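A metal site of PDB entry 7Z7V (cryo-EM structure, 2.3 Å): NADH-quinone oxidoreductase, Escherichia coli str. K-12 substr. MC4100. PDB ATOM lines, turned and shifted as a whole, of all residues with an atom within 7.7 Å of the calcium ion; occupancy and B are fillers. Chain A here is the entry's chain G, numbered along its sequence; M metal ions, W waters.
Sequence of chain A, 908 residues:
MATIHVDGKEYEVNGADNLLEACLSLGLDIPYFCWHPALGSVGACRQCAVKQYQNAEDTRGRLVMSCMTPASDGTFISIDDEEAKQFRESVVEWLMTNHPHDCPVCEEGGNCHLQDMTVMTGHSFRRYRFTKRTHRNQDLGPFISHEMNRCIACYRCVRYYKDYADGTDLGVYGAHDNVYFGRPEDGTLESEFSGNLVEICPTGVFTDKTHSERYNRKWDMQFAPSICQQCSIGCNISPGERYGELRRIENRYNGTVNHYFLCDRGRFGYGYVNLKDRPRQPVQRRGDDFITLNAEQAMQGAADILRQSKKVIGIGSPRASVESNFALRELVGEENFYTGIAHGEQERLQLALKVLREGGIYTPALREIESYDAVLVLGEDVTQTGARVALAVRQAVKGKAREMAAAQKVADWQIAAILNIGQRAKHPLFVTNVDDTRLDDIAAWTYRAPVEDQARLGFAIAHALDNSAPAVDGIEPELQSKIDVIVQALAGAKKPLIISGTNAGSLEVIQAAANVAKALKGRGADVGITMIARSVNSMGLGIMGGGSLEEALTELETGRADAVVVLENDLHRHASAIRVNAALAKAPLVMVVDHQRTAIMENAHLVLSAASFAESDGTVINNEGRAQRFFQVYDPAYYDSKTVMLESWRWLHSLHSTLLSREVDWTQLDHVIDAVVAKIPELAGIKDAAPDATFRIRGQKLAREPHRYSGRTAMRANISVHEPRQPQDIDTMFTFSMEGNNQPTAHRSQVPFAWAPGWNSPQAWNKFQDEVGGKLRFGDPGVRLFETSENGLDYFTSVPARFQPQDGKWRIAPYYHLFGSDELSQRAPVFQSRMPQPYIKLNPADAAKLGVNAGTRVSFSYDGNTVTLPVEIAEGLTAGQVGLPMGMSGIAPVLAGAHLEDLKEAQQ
The side-chain carboxylate of Glu 647 lies within salt-bridge range of the guanidinium group of Arg 650. The backbone NH (N) of Asp 731 lies close to the side-chain carboxylate (OD1) of Asp 729, at 3.3 Å. The backbone NH (N) of Leu 669 is in hydrogen-bond range of the side-chain carboxylate (OD1) of Asp 731 (3.2 Å). The backbone NH (N) of Gln 632 is in hydrogen-bond range of the backbone carbonyl oxygen (O) of Ser 616. O of Gln 632 is in hydrogen-bond range of NE of Arg 704 (2.6 Å). The side-chain amide nitrogen (NE2) of Gln 632 sits at hydrogen-bond distance from the backbone carbonyl oxygen (O) of Tyr 634 (2.7 Å). The side-chain carboxylate of Asp 729 is in hydrogen-bond range of the backbone NH of Thr 732 (3.5 Å). NH2 of Arg 704 is in salt-bridge range of OD2 of Asp 729 (2.9 Å).
OD1 of Asp 729 touches the calcium ion, 3.9 Å away. Of the 20 residues printed, 5 come within 4 Å of the calcium ion. The nearest printed residue that does not touch the calcium ion is Arg 650 (4.2 Å).
The calcium ion is bound by OD2 of Asp 617, OE2 of Glu 647, water W1, OD2 of Asp 731, OE1 of Gln 632 and water W2. The calcium ion has six donor atoms within binding distance.
Water W2 lies within hydrogen-bond range of the side-chain carboxylate (OD1) of Asp 729, the side-chain carboxylate (OD1) of Asp 617 and the guanidinium group (NH2) of Arg 704.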
ATOM      1  N   GLU A 615      -5.845 -14.958  -3.305  1.00  0.00           N
ATOM      2  CA  GLU A 615      -5.269 -14.617  -2.010  1.00  0.00           C
ATOM      3  C   GLU A 615      -6.329 -14.452  -0.926  1.00  0.00           C
ATOM      4  O   GLU A 615      -6.052 -13.834   0.113  1.00  0.00           O
ATOM      5  CB  GLU A 615      -4.439 -13.339  -2.137  1.00  0.00           C
ATOM      6  CG  GLU A 615      -3.384 -13.405  -3.212  1.00  0.00           C
ATOM      7  CD  GLU A 615      -3.674 -12.498  -4.377  1.00  0.00           C
ATOM      8  OE1 GLU A 615      -4.793 -11.975  -4.468  1.00  0.00           O
ATOM      9  OE2 GLU A 615      -2.772 -12.307  -5.224  1.00  0.00           O
ATOM     10  N   SER A 616      -7.532 -14.984  -1.128  1.00  0.00           N
ATOM     11  CA  SER A 616      -8.603 -14.764  -0.171  1.00  0.00           C
ATOM     12  C   SER A 616      -9.501 -15.994  -0.099  1.00  0.00           C
ATOM     13  O   SER A 616      -9.494 -16.848  -0.984  1.00  0.00           O
ATOM     14  CB  SER A 616      -9.440 -13.534  -0.543  1.00  0.00           C
ATOM     15  OG  SER A 616     -10.001 -13.660  -1.827  1.00  0.00           O
ATOM     16  N   ASP A 617     -10.260 -16.064   0.984  1.00  0.00           N
ATOM     17  CA  ASP A 617     -11.315 -17.045   1.158  1.00  0.00           C
ATOM     18  C   ASP A 617     -12.655 -16.344   1.173  1.00  0.00           C
ATOM     19  O   ASP A 617     -12.749 -15.146   1.468  1.00  0.00           O
ATOM     20  CB  ASP A 617     -11.127 -17.835   2.454  1.00  0.00           C
ATOM     21  CG  ASP A 617      -9.687 -18.139   2.753  1.00  0.00           C
ATOM     22  OD1 ASP A 617      -9.186 -19.183   2.292  1.00  0.00           O
ATOM     23  OD2 ASP A 617      -9.047 -17.343   3.452  1.00  0.00           O
ATOM     24  N   GLY A 618     -13.708 -17.084   0.860  1.00  0.00           N
ATOM     25  CA  GLY A 618     -15.032 -16.507   0.915  1.00  0.00           C
ATOM     26  C   GLY A 618     -16.066 -17.439   0.318  1.00  0.00           C
ATOM     27  O   GLY A 618     -15.774 -18.596   0.008  1.00  0.00           O
ATOM     28  N   PHE A 631     -11.219 -21.049  -1.323  1.00  0.00           N
ATOM     29  CA  PHE A 631     -10.161 -21.041  -0.330  1.00  0.00           C
ATOM     30  C   PHE A 631      -8.940 -20.326  -0.891  1.00  0.00           C
ATOM     31  O   PHE A 631      -8.718 -20.315  -2.099  1.00  0.00           O
ATOM     32  CB  PHE A 631      -9.798 -22.470   0.085  1.00  0.00           C
ATOM     33  CG  PHE A 631     -10.960 -23.265   0.648  1.00  0.00           C
ATOM     34  CD1 PHE A 631     -11.825 -23.950  -0.193  1.00  0.00           C
ATOM     35  CD2 PHE A 631     -11.176 -23.331   2.007  1.00  0.00           C
ATOM     36  CE1 PHE A 631     -12.883 -24.667   0.316  1.00  0.00           C
ATOM     37  CE2 PHE A 631     -12.228 -24.053   2.521  1.00  0.00           C
ATOM     38  CZ  PHE A 631     -13.078 -24.727   1.674  1.00  0.00           C
ATOM     39  N   GLN A 632      -8.165 -19.736   0.007  1.00  0.00           N
ATOM     40  CA  GLN A 632      -6.965 -19.011  -0.384  1.00  0.00           C
ATOM     41  C   GLN A 632      -5.921 -19.970  -0.963  1.00  0.00           C
ATOM     42  O   GLN A 632      -5.710 -21.063  -0.438  1.00  0.00           O
ATOM     43  CB  GLN A 632      -6.391 -18.259   0.809  1.00  0.00           C
ATOM     44  CG  GLN A 632      -5.155 -17.446   0.512  1.00  0.00           C
ATOM     45  CD  GLN A 632      -4.764 -16.554   1.667  1.00  0.00           C
ATOM     46  OE1 GLN A 632      -5.496 -16.417   2.638  1.00  0.00           O
ATOM     47  NE2 GLN A 632      -3.587 -15.943   1.574  1.00  0.00           N
ATOM     48  N   VAL A 633      -5.277 -19.554  -2.053  1.00  0.00           N
ATOM     49  CA  VAL A 633      -4.285 -20.392  -2.705  1.00  0.00           C
ATOM     50  C   VAL A 633      -2.914 -20.229  -2.056  1.00  0.00           C
ATOM     51  O   VAL A 633      -2.241 -21.217  -1.750  1.00  0.00           O
ATOM     52  CB  VAL A 633      -4.224 -20.088  -4.215  1.00  0.00           C
ATOM     53  CG1 VAL A 633      -3.382 -21.121  -4.924  1.00  0.00           C
ATOM     54  CG2 VAL A 633      -5.623 -20.066  -4.785  1.00  0.00           C
ATOM     55  N   TYR A 634      -2.484 -18.996  -1.817  1.00  0.00           N
ATOM     56  CA  TYR A 634      -1.147 -18.745  -1.327  1.00  0.00           C
ATOM     57  C   TYR A 634      -1.145 -17.504  -0.455  1.00  0.00           C
ATOM     58  O   TYR A 634      -2.074 -16.698  -0.486  1.00  0.00           O
ATOM     59  CB  TYR A 634      -0.145 -18.585  -2.481  1.00  0.00           C
ATOM     60  CG  TYR A 634      -0.295 -17.292  -3.249  1.00  0.00           C
ATOM     61  CD1 TYR A 634      -1.304 -17.123  -4.180  1.00  0.00           C
ATOM     62  CD2 TYR A 634       0.586 -16.231  -3.042  1.00  0.00           C
ATOM     63  CE1 TYR A 634      -1.444 -15.948  -4.876  1.00  0.00           C
ATOM     64  CE2 TYR A 634       0.453 -15.050  -3.741  1.00  0.00           C
ATOM     65  CZ  TYR A 634      -0.565 -14.914  -4.660  1.00  0.00           C
ATOM     66  OH  TYR A 634      -0.714 -13.744  -5.352  1.00  0.00           O
ATOM     67  N   ASP A 635      -0.084 -17.375   0.336  1.00  0.00           N
ATOM     68  CA  ASP A 635       0.119 -16.177   1.144  1.00  0.00           C
ATOM     69  C   ASP A 635       0.869 -15.136   0.313  1.00  0.00           C
ATOM     70  O   ASP A 635       2.007 -15.395  -0.097  1.00  0.00           O
ATOM     71  CB  ASP A 635       0.907 -16.502   2.390  1.00  0.00           C
ATOM     72  CG  ASP A 635       0.699 -15.490   3.496  1.00  0.00           C
ATOM     73  OD1 ASP A 635       1.014 -14.298   3.283  1.00  0.00           O
ATOM     74  OD2 ASP A 635       0.208 -15.871   4.578  1.00  0.00           O
ATOM     75  N   GLU A 647      -7.932 -10.007   2.956  1.00  0.00           N
ATOM     76  CA  GLU A 647      -9.298 -10.221   2.495  1.00  0.00           C
ATOM     77  C   GLU A 647     -10.118  -8.963   2.734  1.00  0.00           C
ATOM     78  O   GLU A 647      -9.884  -8.212   3.681  1.00  0.00           O
ATOM     79  CB  GLU A 647      -9.926 -11.399   3.243  1.00  0.00           C
ATOM     80  CG  GLU A 647      -9.295 -12.743   2.952  1.00  0.00           C
ATOM     81  CD  GLU A 647      -8.186 -13.090   3.908  1.00  0.00           C
ATOM     82  OE1 GLU A 647      -7.698 -12.201   4.628  1.00  0.00           O
ATOM     83  OE2 GLU A 647      -7.776 -14.271   3.933  1.00  0.00           O
ATOM     84  N   TRP A 649     -13.306  -8.706   3.552  1.00  0.00           N
ATOM     85  CA  TRP A 649     -14.060  -8.807   4.792  1.00  0.00           C
ATOM     86  C   TRP A 649     -13.169  -8.583   6.005  1.00  0.00           C
ATOM     87  O   TRP A 649     -13.627  -8.026   7.007  1.00  0.00           O
ATOM     88  CB  TRP A 649     -14.775 -10.148   4.892  1.00  0.00           C
ATOM     89  CG  TRP A 649     -13.923 -11.352   4.602  1.00  0.00           C
ATOM     90  CD1 TRP A 649     -13.791 -11.988   3.407  1.00  0.00           C
ATOM     91  CD2 TRP A 649     -13.106 -12.066   5.544  1.00  0.00           C
ATOM     92  NE1 TRP A 649     -12.936 -13.048   3.539  1.00  0.00           N
ATOM     93  CE2 TRP A 649     -12.496 -13.118   4.838  1.00  0.00           C
ATOM     94  CE3 TRP A 649     -12.821 -11.914   6.902  1.00  0.00           C
ATOM     95  CZ2 TRP A 649     -11.621 -14.015   5.445  1.00  0.00           C
ATOM     96  CZ3 TRP A 649     -11.958 -12.800   7.497  1.00  0.00           C
ATOM     97  CH2 TRP A 649     -11.366 -13.836   6.774  1.00  0.00           C
ATOM     98  N   ARG A 650     -11.892  -8.972   5.916  1.00  0.00           N
ATOM     99  CA  ARG A 650     -10.954  -8.715   7.007  1.00  0.00           C
ATOM    100  C   ARG A 650     -10.696  -7.233   7.174  1.00  0.00           C
ATOM    101  O   ARG A 650     -10.744  -6.700   8.288  1.00  0.00           O
ATOM    102  CB  ARG A 650      -9.658  -9.478   6.757  1.00  0.00           C
ATOM    103  CG  ARG A 650      -8.614  -9.320   7.835  1.00  0.00           C
ATOM    104  CD  ARG A 650      -7.659 -10.492   7.844  1.00  0.00           C
ATOM    105  NE  ARG A 650      -8.125 -11.569   8.703  1.00  0.00           N
ATOM    106  CZ  ARG A 650      -8.156 -12.853   8.358  1.00  0.00           C
ATOM    107  NH1 ARG A 650      -7.768 -13.256   7.160  1.00  0.00           N
ATOM    108  NH2 ARG A 650      -8.579 -13.749   9.236  1.00  0.00           N
ATOM    109  N   LEU A 669     -12.514 -16.147   9.439  1.00  0.00           N
ATOM    110  CA  LEU A 669     -13.519 -16.309   8.386  1.00  0.00           C
ATOM    111  C   LEU A 669     -14.811 -16.921   8.927  1.00  0.00           C
ATOM    112  O   LEU A 669     -15.911 -16.503   8.545  1.00  0.00           O
ATOM    113  CB  LEU A 669     -12.954 -17.152   7.248  1.00  0.00           C
ATOM    114  CG  LEU A 669     -13.966 -17.609   6.187  1.00  0.00           C
ATOM    115  CD1 LEU A 669     -14.449 -16.439   5.366  1.00  0.00           C
ATOM    116  CD2 LEU A 669     -13.377 -18.690   5.304  1.00  0.00           C
ATOM    117  N   ARG A 704      -2.338 -28.183   0.892  1.00  0.00           N
ATOM    118  CA  ARG A 704      -2.479 -27.376  -0.315  1.00  0.00           C
ATOM    119  C   ARG A 704      -1.513 -27.773  -1.413  1.00  0.00           C
ATOM    120  O   ARG A 704      -1.766 -27.485  -2.587  1.00  0.00           O
ATOM    121  CB  ARG A 704      -2.280 -25.896  -0.002  1.00  0.00           C
ATOM    122  CG  ARG A 704      -3.542 -25.158   0.395  1.00  0.00           C
ATOM    123  CD  ARG A 704      -3.290 -23.667   0.422  1.00  0.00           C
ATOM    124  NE  ARG A 704      -4.469 -22.910   0.835  1.00  0.00           N
ATOM    125  CZ  ARG A 704      -4.785 -22.648   2.085  1.00  0.00           C
ATOM    126  NH1 ARG A 704      -4.032 -23.064   3.096  1.00  0.00           N
ATOM    127  NH2 ARG A 704      -5.879 -21.947   2.340  1.00  0.00           N
ATOM    128  N   GLN A 728       0.571 -19.359   8.263  1.00  0.00           N
ATOM    129  CA  GLN A 728      -0.485 -19.965   9.062  1.00  0.00           C
ATOM    130  C   GLN A 728      -1.835 -19.632   8.470  1.00  0.00           C
ATOM    131  O   GLN A 728      -2.089 -18.498   8.046  1.00  0.00           O
ATOM    132  CB  GLN A 728      -0.391 -19.490  10.506  1.00  0.00           C
ATOM    133  CG  GLN A 728       0.879 -19.932  11.221  1.00  0.00           C
ATOM    134  CD  GLN A 728       1.192 -21.401  11.014  1.00  0.00           C
ATOM    135  OE1 GLN A 728       0.525 -22.273  11.568  1.00  0.00           O
ATOM    136  NE2 GLN A 728       2.210 -21.680  10.212  1.00  0.00           N
ATOM    137  N   ASP A 729      -2.718 -20.619   8.439  1.00  0.00           N
ATOM    138  CA  ASP A 729      -4.071 -20.461   7.912  1.00  0.00           C
ATOM    139  C   ASP A 729      -5.051 -20.650   9.068  1.00  0.00           C
ATOM    140  O   ASP A 729      -5.467 -21.762   9.376  1.00  0.00           O
ATOM    141  CB  ASP A 729      -4.335 -21.443   6.781  1.00  0.00           C
ATOM    142  CG  ASP A 729      -5.615 -21.132   6.026  1.00  0.00           C
ATOM    143  OD1 ASP A 729      -6.162 -20.025   6.215  1.00  0.00           O
ATOM    144  OD2 ASP A 729      -6.063 -21.983   5.245  1.00  0.00           O
ATOM    145  N   ILE A 730      -5.417 -19.542   9.704  1.00  0.00           N
ATOM    146  CA  ILE A 730      -6.440 -19.595  10.739  1.00  0.00           C
ATOM    147  C   ILE A 730      -7.843 -19.591  10.157  1.00  0.00           C
ATOM    148  O   ILE A 730      -8.798 -19.942  10.860  1.00  0.00           O
ATOM    149  CB  ILE A 730      -6.294 -18.420  11.724  1.00  0.00           C
ATOM    150  CG1 ILE A 730      -6.488 -17.086  10.991  1.00  0.00           C
ATOM    151  CG2 ILE A 730      -4.942 -18.458  12.415  1.00  0.00           C
ATOM    152  CD1 ILE A 730      -6.937 -15.962  11.885  1.00  0.00           C
ATOM    153  N   ASP A 731      -7.998 -19.240   8.887  1.00  0.00           N
ATOM    154  CA  ASP A 731      -9.322 -19.055   8.318  1.00  0.00           C
ATOM    155  C   ASP A 731      -9.972 -20.381   7.934  1.00  0.00           C
ATOM    156  O   ASP A 731     -11.177 -20.553   8.119  1.00  0.00           O
ATOM    157  CB  ASP A 731      -9.248 -18.137   7.107  1.00  0.00           C
ATOM    158  CG  ASP A 731      -8.948 -16.704   7.495  1.00  0.00           C
ATOM    159  OD1 ASP A 731      -9.430 -16.264   8.549  1.00  0.00           O
ATOM    160  OD2 ASP A 731      -8.222 -16.028   6.748  1.00  0.00           O
ATOM    161  N   THR A 732      -9.206 -21.307   7.370  1.00  0.00           N
ATOM    162  CA  THR A 732      -9.755 -22.513   6.766  1.00  0.00           C
ATOM    163  C   THR A 732      -9.074 -23.750   7.332  1.00  0.00           C
ATOM    164  O   THR A 732      -8.136 -23.680   8.130  1.00  0.00           O
ATOM    165  CB  THR A 732      -9.626 -22.505   5.238  1.00  0.00           C
ATOM    166  OG1 THR A 732      -8.255 -22.650   4.878  1.00  0.00           O
ATOM    167  CG2 THR A 732     -10.168 -21.205   4.652  1.00  0.00           C
ATOM    168  N   PHE A 736      -0.862 -24.252   4.472  1.00  0.00           N
ATOM    169  CA  PHE A 736       0.018 -23.733   3.416  1.00  0.00           C
ATOM    170  C   PHE A 736       1.316 -24.549   3.341  1.00  0.00           C
ATOM    171  O   PHE A 736       2.420 -24.010   3.397  1.00  0.00           O
ATOM    172  CB  PHE A 736       0.319 -22.269   3.660  1.00  0.00           C
ATOM    173  CG  PHE A 736      -0.827 -21.347   3.380  1.00  0.00           C
ATOM    174  CD1 PHE A 736      -1.277 -21.156   2.083  1.00  0.00           C
ATOM    175  CD2 PHE A 736      -1.445 -20.651   4.403  1.00  0.00           C
ATOM    176  CE1 PHE A 736      -2.330 -20.302   1.814  1.00  0.00           C
ATOM    177  CE2 PHE A 736      -2.494 -19.797   4.147  1.00  0.00           C
ATOM    178  CZ  PHE A 736      -2.937 -19.628   2.858  1.00  0.00           C
HETATM  179 CA    CA M   1      -7.049 -16.542   4.598  1.00  0.00          CA
HETATM  180  O   HOH W   1      -5.068 -15.346   5.506  1.00  0.00           O
HETATM  181  O   HOH W   2      -6.815 -19.069   4.047  1.00  0.00           O
